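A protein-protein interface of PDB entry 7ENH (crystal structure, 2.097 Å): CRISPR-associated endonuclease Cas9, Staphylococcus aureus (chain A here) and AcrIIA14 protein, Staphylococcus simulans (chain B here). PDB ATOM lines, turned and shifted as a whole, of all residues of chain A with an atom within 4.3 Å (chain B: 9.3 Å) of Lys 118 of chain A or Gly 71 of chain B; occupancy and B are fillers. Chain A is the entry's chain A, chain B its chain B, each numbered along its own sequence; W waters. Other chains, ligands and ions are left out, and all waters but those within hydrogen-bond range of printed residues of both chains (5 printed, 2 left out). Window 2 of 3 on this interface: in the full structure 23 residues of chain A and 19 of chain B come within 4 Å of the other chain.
OD1 of Asp 116 of chain A is in salt-bridge range of NZ of Lys 64 of chain B.
The backbone carbonyl oxygen of Ser 117 of chain A is in hydrogen-bond range of the backbone NH of Ile 72 of chain B (3.2 Å).
The backbone NH of Gly 71 of chain B sits at hydrogen-bond distance from the backbone carbonyl oxygen of Ser 115 of chain A (2.9 Å).
The side-chain amide oxygen of Asn 70 of chain B lies within hydrogen-bond range of the backbone NH of Gly 73 of chain B (2.8 Å).
O of Ile 72 of chain B lies within hydrogen-bond range of NZ of Lys 93 of chain B.
The side-chain amide oxygen (OD1) of Asn 70 of chain B is in hydrogen-bond range of the backbone NH (N) of Ile 72 of chain B.
O of Ser 8 of chain B is in hydrogen-bond range of ND2 of Asn 70 of chain B (2.9 Å).
The side-chain hydroxyl (OG) of Ser 117 of chain A is in hydrogen-bond range of the backbone carbonyl oxygen (O) of Ile 119 of chain A (3.2 Å).
The side-chain amino group (NZ) of Lys 118 of chain A is in salt-bridge range of the side-chain carboxylate (OE1) of Glu 59 of chain A (3.2 Å).
Ser 115 of chain A touches Ser 8 of chain B (CB to CB, 3.6 Å).
Asn 22 of chain B touches Ser 115 of chain A.
Asn 70 of chain B touches Ser 115 of chain A.
Gly 71 of chain B touches Ser 117 of chain A.
Lys 118 of chain A touches Gly 71 of chain B.
O of Lys 118 of chain A touches CG1 of Ile 72 of chain B (3.7 Å).
C of Ile 119 of chain A touches CD1 of Ile 72 of chain B (3.6 Å).
Glu 98 of chain A touches none of the printed residues of chain B.
Of the printed residues of chain B, Asp 116 of chain A touches Lys 64 (2.7 Å).
Of chain B, only Gly 71 (3.7 Å) and Ile 72 (3.7 Å) come within 4 Å of Lys 118 of chain A.
Of the printed residues of chain A, Ser 8 of chain B touches Ser 115 (3.6 Å).
Of chain A, only Ser 115 (2.9 Å), Ser 117 (3.1 Å) and Lys 118 (3.7 Å) come within 4 Å of Gly 71 of chain B.
Tyr 74 of chain B touches none of the printed residues of chain A.
The nearest residue of chain B that does not touch Lys 118 of chain A is Asn 97 of chain B (5.3 Å).
The nearest printed residue of chain A that does not touch Gly 71 of chain B is Asp 116 of chain A (4.8 Å).
Among the printed residues, 10 pairs touch across the chains.
Among the printed residues, Asp or Glu carboxylates within 4 Å of a Lys or Arg side-chain nitrogen of the other chain: Asp 116 of chain A with Lys 64 of chain B (2.7 Å).
Water W5 lies within hydrogen-bond range of OG of Ser 115 of chain A (2.7 Å), OD1 of Asp 116 of chain A (3.1 Å) and ND2 of Asn 22 of chain B (3.2 Å).
Water W3 lies within hydrogen-bond range of OG of Ser 115 of chain A, OG of Ser 8 of chain B and OD1 of Asn 22 of chain B.
Water W4 bridges the backbone carbonyl oxygen (O) of Lys 118 of chain A (2.7 Å) and the backbone carbonyl oxygen (O) of Gly 71 of chain B (3.1 Å).
Water W1 lies within hydrogen-bond range of the backbone carbonyl oxygen (O) of Ser 117 of chain A, the backbone carbonyl oxygen (O) of Ser 115 of chain A, the backbone NH (N) of Gly 71 of chain B and the backbone NH (N) of Ile 72 of chain B.
Water W2 lies within hydrogen-bond range of NZ of Lys 64 of chain B (2.9 Å), OG of Ser 115 of chain A (3.1 Å) and ND2 of Asn 22 of chain B (3.2 Å).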
ATOM      1  N   GLU A  59      -2.088   4.451   3.921  1.00  0.00           N
ATOM      2  CA  GLU A  59      -1.068   5.463   3.704  1.00  0.00           C
ATOM      3  C   GLU A  59      -1.670   6.647   2.961  1.00  0.00           C
ATOM      4  O   GLU A  59      -2.640   6.509   2.211  1.00  0.00           O
ATOM      5  CB  GLU A  59       0.109   4.890   2.913  1.00  0.00           C
ATOM      6  CG  GLU A  59       0.935   3.866   3.675  1.00  0.00           C
ATOM      7  CD  GLU A  59       2.042   3.265   2.830  1.00  0.00           C
ATOM      8  OE1 GLU A  59       2.578   2.206   3.218  1.00  0.00           O
ATOM      9  OE2 GLU A  59       2.376   3.851   1.779  1.00  0.00           O
ATOM     10  N   GLU A  98       1.338  -0.758  -6.089  1.00  0.00           N
ATOM     11  CA  GLU A  98       1.862  -1.989  -5.501  1.00  0.00           C
ATOM     12  C   GLU A  98       0.798  -2.730  -4.700  1.00  0.00           C
ATOM     13  O   GLU A  98       0.778  -3.967  -4.681  1.00  0.00           O
ATOM     14  CB  GLU A  98       3.074  -1.669  -4.622  1.00  0.00           C
ATOM     15  CG  GLU A  98       2.781  -0.755  -3.439  1.00  0.00           C
ATOM     16  CD  GLU A  98       3.788  -0.921  -2.318  1.00  0.00           C
ATOM     17  OE1 GLU A  98       4.588  -1.876  -2.382  1.00  0.00           O
ATOM     18  OE2 GLU A  98       3.788  -0.097  -1.378  1.00  0.00           O
ATOM     19  N   GLU A  99      -0.094  -1.996  -4.033  1.00  0.00           N
ATOM     20  CA  GLU A  99      -1.146  -2.647  -3.257  1.00  0.00           C
ATOM     21  C   GLU A  99      -2.126  -3.378  -4.164  1.00  0.00           C
ATOM     22  O   GLU A  99      -2.551  -4.499  -3.859  1.00  0.00           O
ATOM     23  CB  GLU A  99      -1.873  -1.618  -2.395  1.00  0.00           C
ATOM     24  CG  GLU A  99      -1.027  -1.033  -1.277  1.00  0.00           C
ATOM     25  CD  GLU A  99      -0.613  -2.077  -0.259  1.00  0.00           C
ATOM     26  OE1 GLU A  99      -1.479  -2.871   0.167  1.00  0.00           O
ATOM     27  OE2 GLU A  99       0.577  -2.107   0.115  1.00  0.00           O
ATOM     28  N   LYS A 102      -0.239  -6.554  -5.245  1.00  0.00           N
ATOM     29  CA  LYS A 102      -0.172  -7.571  -4.218  1.00  0.00           C
ATOM     30  C   LYS A 102      -1.526  -8.234  -3.929  1.00  0.00           C
ATOM     31  O   LYS A 102      -1.588  -9.418  -3.676  1.00  0.00           O
ATOM     32  CB  LYS A 102       0.417  -7.015  -2.925  1.00  0.00           C
ATOM     33  CG  LYS A 102       1.907  -6.730  -2.985  1.00  0.00           C
ATOM     34  CD  LYS A 102       2.441  -6.173  -1.686  1.00  0.00           C
ATOM     35  CE  LYS A 102       1.692  -4.928  -1.254  1.00  0.00           C
ATOM     36  NZ  LYS A 102       1.910  -4.534   0.165  1.00  0.00           N
ATOM     37  N   SER A 115       0.332 -12.442   4.591  1.00  0.00           N
ATOM     38  CA  SER A 115       1.594 -11.823   4.960  1.00  0.00           C
ATOM     39  C   SER A 115       2.019 -10.764   3.955  1.00  0.00           C
ATOM     40  O   SER A 115       3.088 -10.168   4.115  1.00  0.00           O
ATOM     41  CB  SER A 115       2.689 -12.888   5.092  1.00  0.00           C
ATOM     42  OG  SER A 115       2.888 -13.564   3.863  1.00  0.00           O
ATOM     43  N   ASP A 116       1.208 -10.518   2.924  1.00  0.00           N
ATOM     44  CA  ASP A 116       1.530  -9.563   1.873  1.00  0.00           C
ATOM     45  C   ASP A 116       1.076  -8.142   2.187  1.00  0.00           C
ATOM     46  O   ASP A 116       1.487  -7.207   1.489  1.00  0.00           O
ATOM     47  CB  ASP A 116       0.896 -10.004   0.547  1.00  0.00           C
ATOM     48  CG  ASP A 116       1.228 -11.441   0.186  1.00  0.00           C
ATOM     49  OD1 ASP A 116       2.280 -11.944   0.632  1.00  0.00           O
ATOM     50  OD2 ASP A 116       0.429 -12.071  -0.539  1.00  0.00           O
ATOM     51  N   SER A 117       0.252  -7.952   3.211  1.00  0.00           N
ATOM     52  CA  SER A 117      -0.355  -6.660   3.483  1.00  0.00           C
ATOM     53  C   SER A 117       0.479  -5.852   4.471  1.00  0.00           C
ATOM     54  O   SER A 117       1.256  -6.395   5.258  1.00  0.00           O
ATOM     55  CB  SER A 117      -1.769  -6.839   4.028  1.00  0.00           C
ATOM     56  OG  SER A 117      -1.750  -7.485   5.291  1.00  0.00           O
ATOM     57  N   LYS A 118       0.284  -4.534   4.433  1.00  0.00           N
ATOM     58  CA  LYS A 118       1.001  -3.620   5.313  1.00  0.00           C
ATOM     59  C   LYS A 118       0.243  -3.303   6.595  1.00  0.00           C
ATOM     60  O   LYS A 118       0.863  -2.862   7.570  1.00  0.00           O
ATOM     61  CB  LYS A 118       1.309  -2.312   4.579  1.00  0.00           C
ATOM     62  CG  LYS A 118       2.319  -2.447   3.454  1.00  0.00           C
ATOM     63  CD  LYS A 118       2.577  -1.100   2.798  1.00  0.00           C
ATOM     64  CE  LYS A 118       3.777  -1.154   1.868  1.00  0.00           C
ATOM     65  NZ  LYS A 118       4.115   0.191   1.324  1.00  0.00           N
ATOM     66  N   ILE A 119      -1.075  -3.502   6.618  1.00  0.00           N
ATOM     67  CA  ILE A 119      -1.887  -3.236   7.795  1.00  0.00           C
ATOM     68  C   ILE A 119      -2.737  -4.462   8.093  1.00  0.00           C
ATOM     69  O   ILE A 119      -2.985  -5.304   7.228  1.00  0.00           O
ATOM     70  CB  ILE A 119      -2.788  -1.994   7.622  1.00  0.00           C
ATOM     71  CG1 ILE A 119      -3.779  -2.213   6.478  1.00  0.00           C
ATOM     72  CG2 ILE A 119      -1.946  -0.748   7.389  1.00  0.00           C
ATOM     73  CD1 ILE A 119      -4.858  -1.161   6.396  1.00  0.00           C
ATOM     74  N   SER B   8       2.265 -17.007   9.357  1.00  0.00           N
ATOM     75  CA  SER B   8       2.576 -15.687   8.823  1.00  0.00           C
ATOM     76  C   SER B   8       1.797 -14.559   9.483  1.00  0.00           C
ATOM     77  O   SER B   8       2.293 -13.431   9.532  1.00  0.00           O
ATOM     78  CB  SER B   8       2.311 -15.651   7.313  1.00  0.00           C
ATOM     79  OG  SER B   8       2.850 -16.793   6.673  1.00  0.00           O
ATOM     80  N   ASN B   9       0.598 -14.826   9.991  1.00  0.00           N
ATOM     81  CA  ASN B   9      -0.228 -13.764  10.544  1.00  0.00           C
ATOM     82  C   ASN B   9      -1.224 -14.361  11.526  1.00  0.00           C
ATOM     83  O   ASN B   9      -1.732 -15.464  11.309  1.00  0.00           O
ATOM     84  CB  ASN B   9      -0.966 -13.003   9.437  1.00  0.00           C
ATOM     85  CG  ASN B   9      -1.175 -11.542   9.775  1.00  0.00           C
ATOM     86  OD1 ASN B   9      -1.011 -11.129  10.923  1.00  0.00           O
ATOM     87  ND2 ASN B   9      -1.538 -10.749   8.773  1.00  0.00           N
ATOM     88  N   ASN B  22       1.388 -20.096   5.442  1.00  0.00           N
ATOM     89  CA  ASN B  22       1.937 -20.241   4.100  1.00  0.00           C
ATOM     90  C   ASN B  22       2.669 -21.573   4.009  1.00  0.00           C
ATOM     91  O   ASN B  22       3.582 -21.841   4.797  1.00  0.00           O
ATOM     92  CB  ASN B  22       2.889 -19.091   3.766  1.00  0.00           C
ATOM     93  CG  ASN B  22       2.165 -17.780   3.550  1.00  0.00           C
ATOM     94  OD1 ASN B  22       1.990 -16.996   4.479  1.00  0.00           O
ATOM     95  ND2 ASN B  22       1.738 -17.534   2.316  1.00  0.00           N
ATOM     96  N   LYS B  64       8.197 -16.692  -2.169  1.00  0.00           N
ATOM     97  CA  LYS B  64       9.009 -15.523  -1.877  1.00  0.00           C
ATOM     98  C   LYS B  64      10.472 -15.921  -1.716  1.00  0.00           C
ATOM     99  O   LYS B  64      10.803 -17.065  -1.395  1.00  0.00           O
ATOM    100  CB  LYS B  64       8.513 -14.826  -0.610  1.00  0.00           C
ATOM    101  CG  LYS B  64       7.003 -14.669  -0.530  1.00  0.00           C
ATOM    102  CD  LYS B  64       6.514 -13.535  -1.416  1.00  0.00           C
ATOM    103  CE  LYS B  64       5.052 -13.217  -1.145  1.00  0.00           C
ATOM    104  NZ  LYS B  64       4.803 -12.922   0.293  1.00  0.00           N
ATOM    105  N   ARG B  66      12.331 -14.711   0.580  1.00  0.00           N
ATOM    106  CA  ARG B  66      12.684 -14.507   1.978  1.00  0.00           C
ATOM    107  C   ARG B  66      11.426 -14.651   2.820  1.00  0.00           C
ATOM    108  O   ARG B  66      10.362 -14.154   2.444  1.00  0.00           O
ATOM    109  CB  ARG B  66      13.319 -13.127   2.183  1.00  0.00           C
ATOM    110  CG  ARG B  66      13.933 -12.895   3.551  1.00  0.00           C
ATOM    111  CD  ARG B  66      14.506 -11.488   3.635  1.00  0.00           C
ATOM    112  NE  ARG B  66      15.030 -11.173   4.961  1.00  0.00           N
ATOM    113  CZ  ARG B  66      16.312 -11.259   5.295  1.00  0.00           C
ATOM    114  NH1 ARG B  66      17.208 -11.653   4.402  1.00  0.00           N
ATOM    115  NH2 ARG B  66      16.699 -10.951   6.526  1.00  0.00           N
ATOM    116  N   ASP B  68      11.053 -13.812   6.464  1.00  0.00           N
ATOM    117  CA  ASP B  68      11.518 -13.230   7.719  1.00  0.00           C
ATOM    118  C   ASP B  68      10.364 -12.567   8.457  1.00  0.00           C
ATOM    119  O   ASP B  68       9.927 -13.066   9.498  1.00  0.00           O
ATOM    120  CB  ASP B  68      12.650 -12.238   7.438  1.00  0.00           C
ATOM    121  CG  ASP B  68      13.248 -11.652   8.704  1.00  0.00           C
ATOM    122  OD1 ASP B  68      12.974 -12.178   9.802  1.00  0.00           O
ATOM    123  OD2 ASP B  68      13.997 -10.659   8.596  1.00  0.00           O
ATOM    124  N   LYS B  69       9.851 -11.449   7.949  1.00  0.00           N
ATOM    125  CA  LYS B  69       8.732 -10.748   8.559  1.00  0.00           C
ATOM    126  C   LYS B  69       7.642 -10.539   7.521  1.00  0.00           C
ATOM    127  O   LYS B  69       7.920 -10.407   6.326  1.00  0.00           O
ATOM    128  CB  LYS B  69       9.162  -9.390   9.134  1.00  0.00           C
ATOM    129  CG  LYS B  69      10.150  -9.479  10.284  1.00  0.00           C
ATOM    130  CD  LYS B  69      10.681  -8.102  10.658  1.00  0.00           C
ATOM    131  CE  LYS B  69      11.675  -8.183  11.807  1.00  0.00           C
ATOM    132  NZ  LYS B  69      12.783  -9.136  11.520  1.00  0.00           N
ATOM    133  N   ASN B  70       6.394 -10.512   7.981  1.00  0.00           N
ATOM    134  CA  ASN B  70       5.309 -10.193   7.067  1.00  0.00           C
ATOM    135  C   ASN B  70       5.285  -8.691   6.789  1.00  0.00           C
ATOM    136  O   ASN B  70       6.040  -7.910   7.373  1.00  0.00           O
ATOM    137  CB  ASN B  70       3.967 -10.685   7.612  1.00  0.00           C
ATOM    138  CG  ASN B  70       3.555 -10.009   8.916  1.00  0.00           C
ATOM    139  OD1 ASN B  70       4.109  -8.987   9.321  1.00  0.00           O
ATOM    140  ND2 ASN B  70       2.565 -10.592   9.581  1.00  0.00           N
ATOM    141  N   GLY B  71       4.396  -8.288   5.878  1.00  0.00           N
ATOM    142  CA  GLY B  71       4.301  -6.889   5.501  1.00  0.00           C
ATOM    143  C   GLY B  71       3.958  -5.962   6.647  1.00  0.00           C
ATOM    144  O   GLY B  71       4.304  -4.776   6.600  1.00  0.00           O
ATOM    145  N   ILE B  72       3.287  -6.473   7.679  1.00  0.00           N
ATOM    146  CA  ILE B  72       2.974  -5.651   8.844  1.00  0.00           C
ATOM    147  C   ILE B  72       4.200  -5.476   9.732  1.00  0.00           C
ATOM    148  O   ILE B  72       4.345  -4.448  10.403  1.00  0.00           O
ATOM    149  CB  ILE B  72       1.797  -6.269   9.619  1.00  0.00           C
ATOM    150  CG1 ILE B  72       0.571  -6.387   8.712  1.00  0.00           C
ATOM    151  CG2 ILE B  72       1.460  -5.445  10.856  1.00  0.00           C
ATOM    152  CD1 ILE B  72      -0.619  -7.033   9.381  1.00  0.00           C
ATOM    153  N   GLY B  73       5.101  -6.453   9.743  1.00  0.00           N
ATOM    154  CA  GLY B  73       6.270  -6.422  10.603  1.00  0.00           C
ATOM    155  C   GLY B  73       6.339  -7.551  11.607  1.00  0.00           C
ATOM    156  O   GLY B  73       7.343  -7.654  12.326  1.00  0.00           O
ATOM    157  N   TYR B  74       5.317  -8.399  11.698  1.00  0.00           N
ATOM    158  CA  TYR B  74       5.366  -9.542  12.599  1.00  0.00           C
ATOM    159  C   TYR B  74       6.467 -10.502  12.166  1.00  0.00           C
ATOM    160  O   TYR B  74       6.735 -10.677  10.975  1.00  0.00           O
ATOM    161  CB  TYR B  74       4.026 -10.281  12.615  1.00  0.00           C
ATOM    162  CG  TYR B  74       2.830  -9.462  13.055  1.00  0.00           C
ATOM    163  CD1 TYR B  74       2.985  -8.252  13.719  1.00  0.00           C
ATOM    164  CD2 TYR B  74       1.537  -9.909  12.804  1.00  0.00           C
ATOM    165  CE1 TYR B  74       1.886  -7.510  14.118  1.00  0.00           C
ATOM    166  CE2 TYR B  74       0.436  -9.174  13.198  1.00  0.00           C
ATOM    167  CZ  TYR B  74       0.616  -7.976  13.854  1.00  0.00           C
ATOM    168  OH  TYR B  74      -0.479  -7.244  14.248  1.00  0.00           O
ATOM    169  N   LYS B  75       7.105 -11.132  13.147  1.00  0.00           N
ATOM    170  CA  LYS B  75       8.128 -12.128  12.861  1.00  0.00           C
ATOM    171  C   LYS B  75       7.458 -13.436  12.458  1.00  0.00           C
ATOM    172  O   LYS B  75       6.628 -13.970  13.201  1.00  0.00           O
ATOM    173  CB  LYS B  75       9.035 -12.333  14.072  1.00  0.00           C
ATOM    174  CG  LYS B  75      10.171 -13.312  13.828  1.00  0.00           C
ATOM    175  CD  LYS B  75      11.115 -12.803  12.750  1.00  0.00           C
ATOM    176  CE  LYS B  75      12.194 -13.825  12.433  1.00  0.00           C
ATOM    177  NZ  LYS B  75      11.703 -14.891  11.518  1.00  0.00           N
ATOM    178  N   ILE B  76       7.813 -13.945  11.282  1.00  0.00           N
ATOM    179  CA  ILE B  76       7.238 -15.185  10.777  1.00  0.00           C
ATOM    180  C   ILE B  76       7.943 -16.363  11.434  1.00  0.00           C
ATOM    181  O   ILE B  76       9.178 -16.416  11.481  1.00  0.00           O
ATOM    182  CB  ILE B  76       7.351 -15.252   9.246  1.00  0.00           C
ATOM    183  CG1 ILE B  76       6.484 -14.171   8.598  1.00  0.00           C
ATOM    184  CG2 ILE B  76       6.956 -16.626   8.738  1.00  0.00           C
ATOM    185  CD1 ILE B  76       6.783 -13.950   7.132  1.00  0.00           C
ATOM    186  N   LYS B  93       3.629  -5.833  18.984  1.00  0.00           N
ATOM    187  CA  LYS B  93       3.260  -5.297  17.680  1.00  0.00           C
ATOM    188  C   LYS B  93       1.799  -5.599  17.359  1.00  0.00           C
ATOM    189  O   LYS B  93       1.102  -4.761  16.776  1.00  0.00           O
ATOM    190  CB  LYS B  93       4.179  -5.862  16.601  1.00  0.00           C
ATOM    191  CG  LYS B  93       4.107  -5.116  15.280  1.00  0.00           C
ATOM    192  CD  LYS B  93       5.398  -5.274  14.495  1.00  0.00           C
ATOM    193  CE  LYS B  93       5.907  -3.930  14.009  1.00  0.00           C
ATOM    194  NZ  LYS B  93       4.815  -3.129  13.396  1.00  0.00           N
ATOM    195  N   ASN B  97      -1.626  -3.086  16.292  1.00  0.00           N
ATOM    196  CA  ASN B  97      -2.424  -3.327  15.097  1.00  0.00           C
ATOM    197  C   ASN B  97      -3.774  -3.958  15.417  1.00  0.00           C
ATOM    198  O   ASN B  97      -4.388  -4.573  14.538  1.00  0.00           O
ATOM    199  CB  ASN B  97      -1.652  -4.207  14.113  1.00  0.00           C
ATOM    200  CG  ASN B  97      -0.366  -3.563  13.635  1.00  0.00           C
ATOM    201  OD1 ASN B  97       0.725  -3.901  14.099  1.00  0.00           O
ATOM    202  ND2 ASN B  97      -0.488  -2.627  12.704  1.00  0.00           N
ATOM    203  N   ASP B  99      -4.561  -6.563  16.961  1.00  0.00           N
ATOM    204  CA  ASP B  99      -4.565  -8.013  16.823  1.00  0.00           C
ATOM    205  C   ASP B  99      -4.354  -8.733  18.147  1.00  0.00           C
ATOM    206  O   ASP B  99      -4.277  -9.966  18.161  1.00  0.00           O
ATOM    207  CB  ASP B  99      -3.492  -8.452  15.821  1.00  0.00           C
ATOM    208  CG  ASP B  99      -3.867  -8.132  14.389  1.00  0.00           C
ATOM    209  OD1 ASP B  99      -5.075  -8.139  14.075  1.00  0.00           O
ATOM    210  OD2 ASP B  99      -2.951  -7.874  13.580  1.00  0.00           O
HETATM  211  O   HOH W   1       1.101  -8.889   6.508  1.00  0.00           O
HETATM  212  O   HOH W   2       3.954 -15.369   1.615  1.00  0.00           O
HETATM  213  O   HOH W   3       4.979 -15.184   4.480  1.00  0.00           O
HETATM  214  O   HOH W   4       3.443  -1.970   7.453  1.00  0.00           O
HETATM  215  O   HOH W   5       1.035 -14.376   2.148  1.00  0.00           O
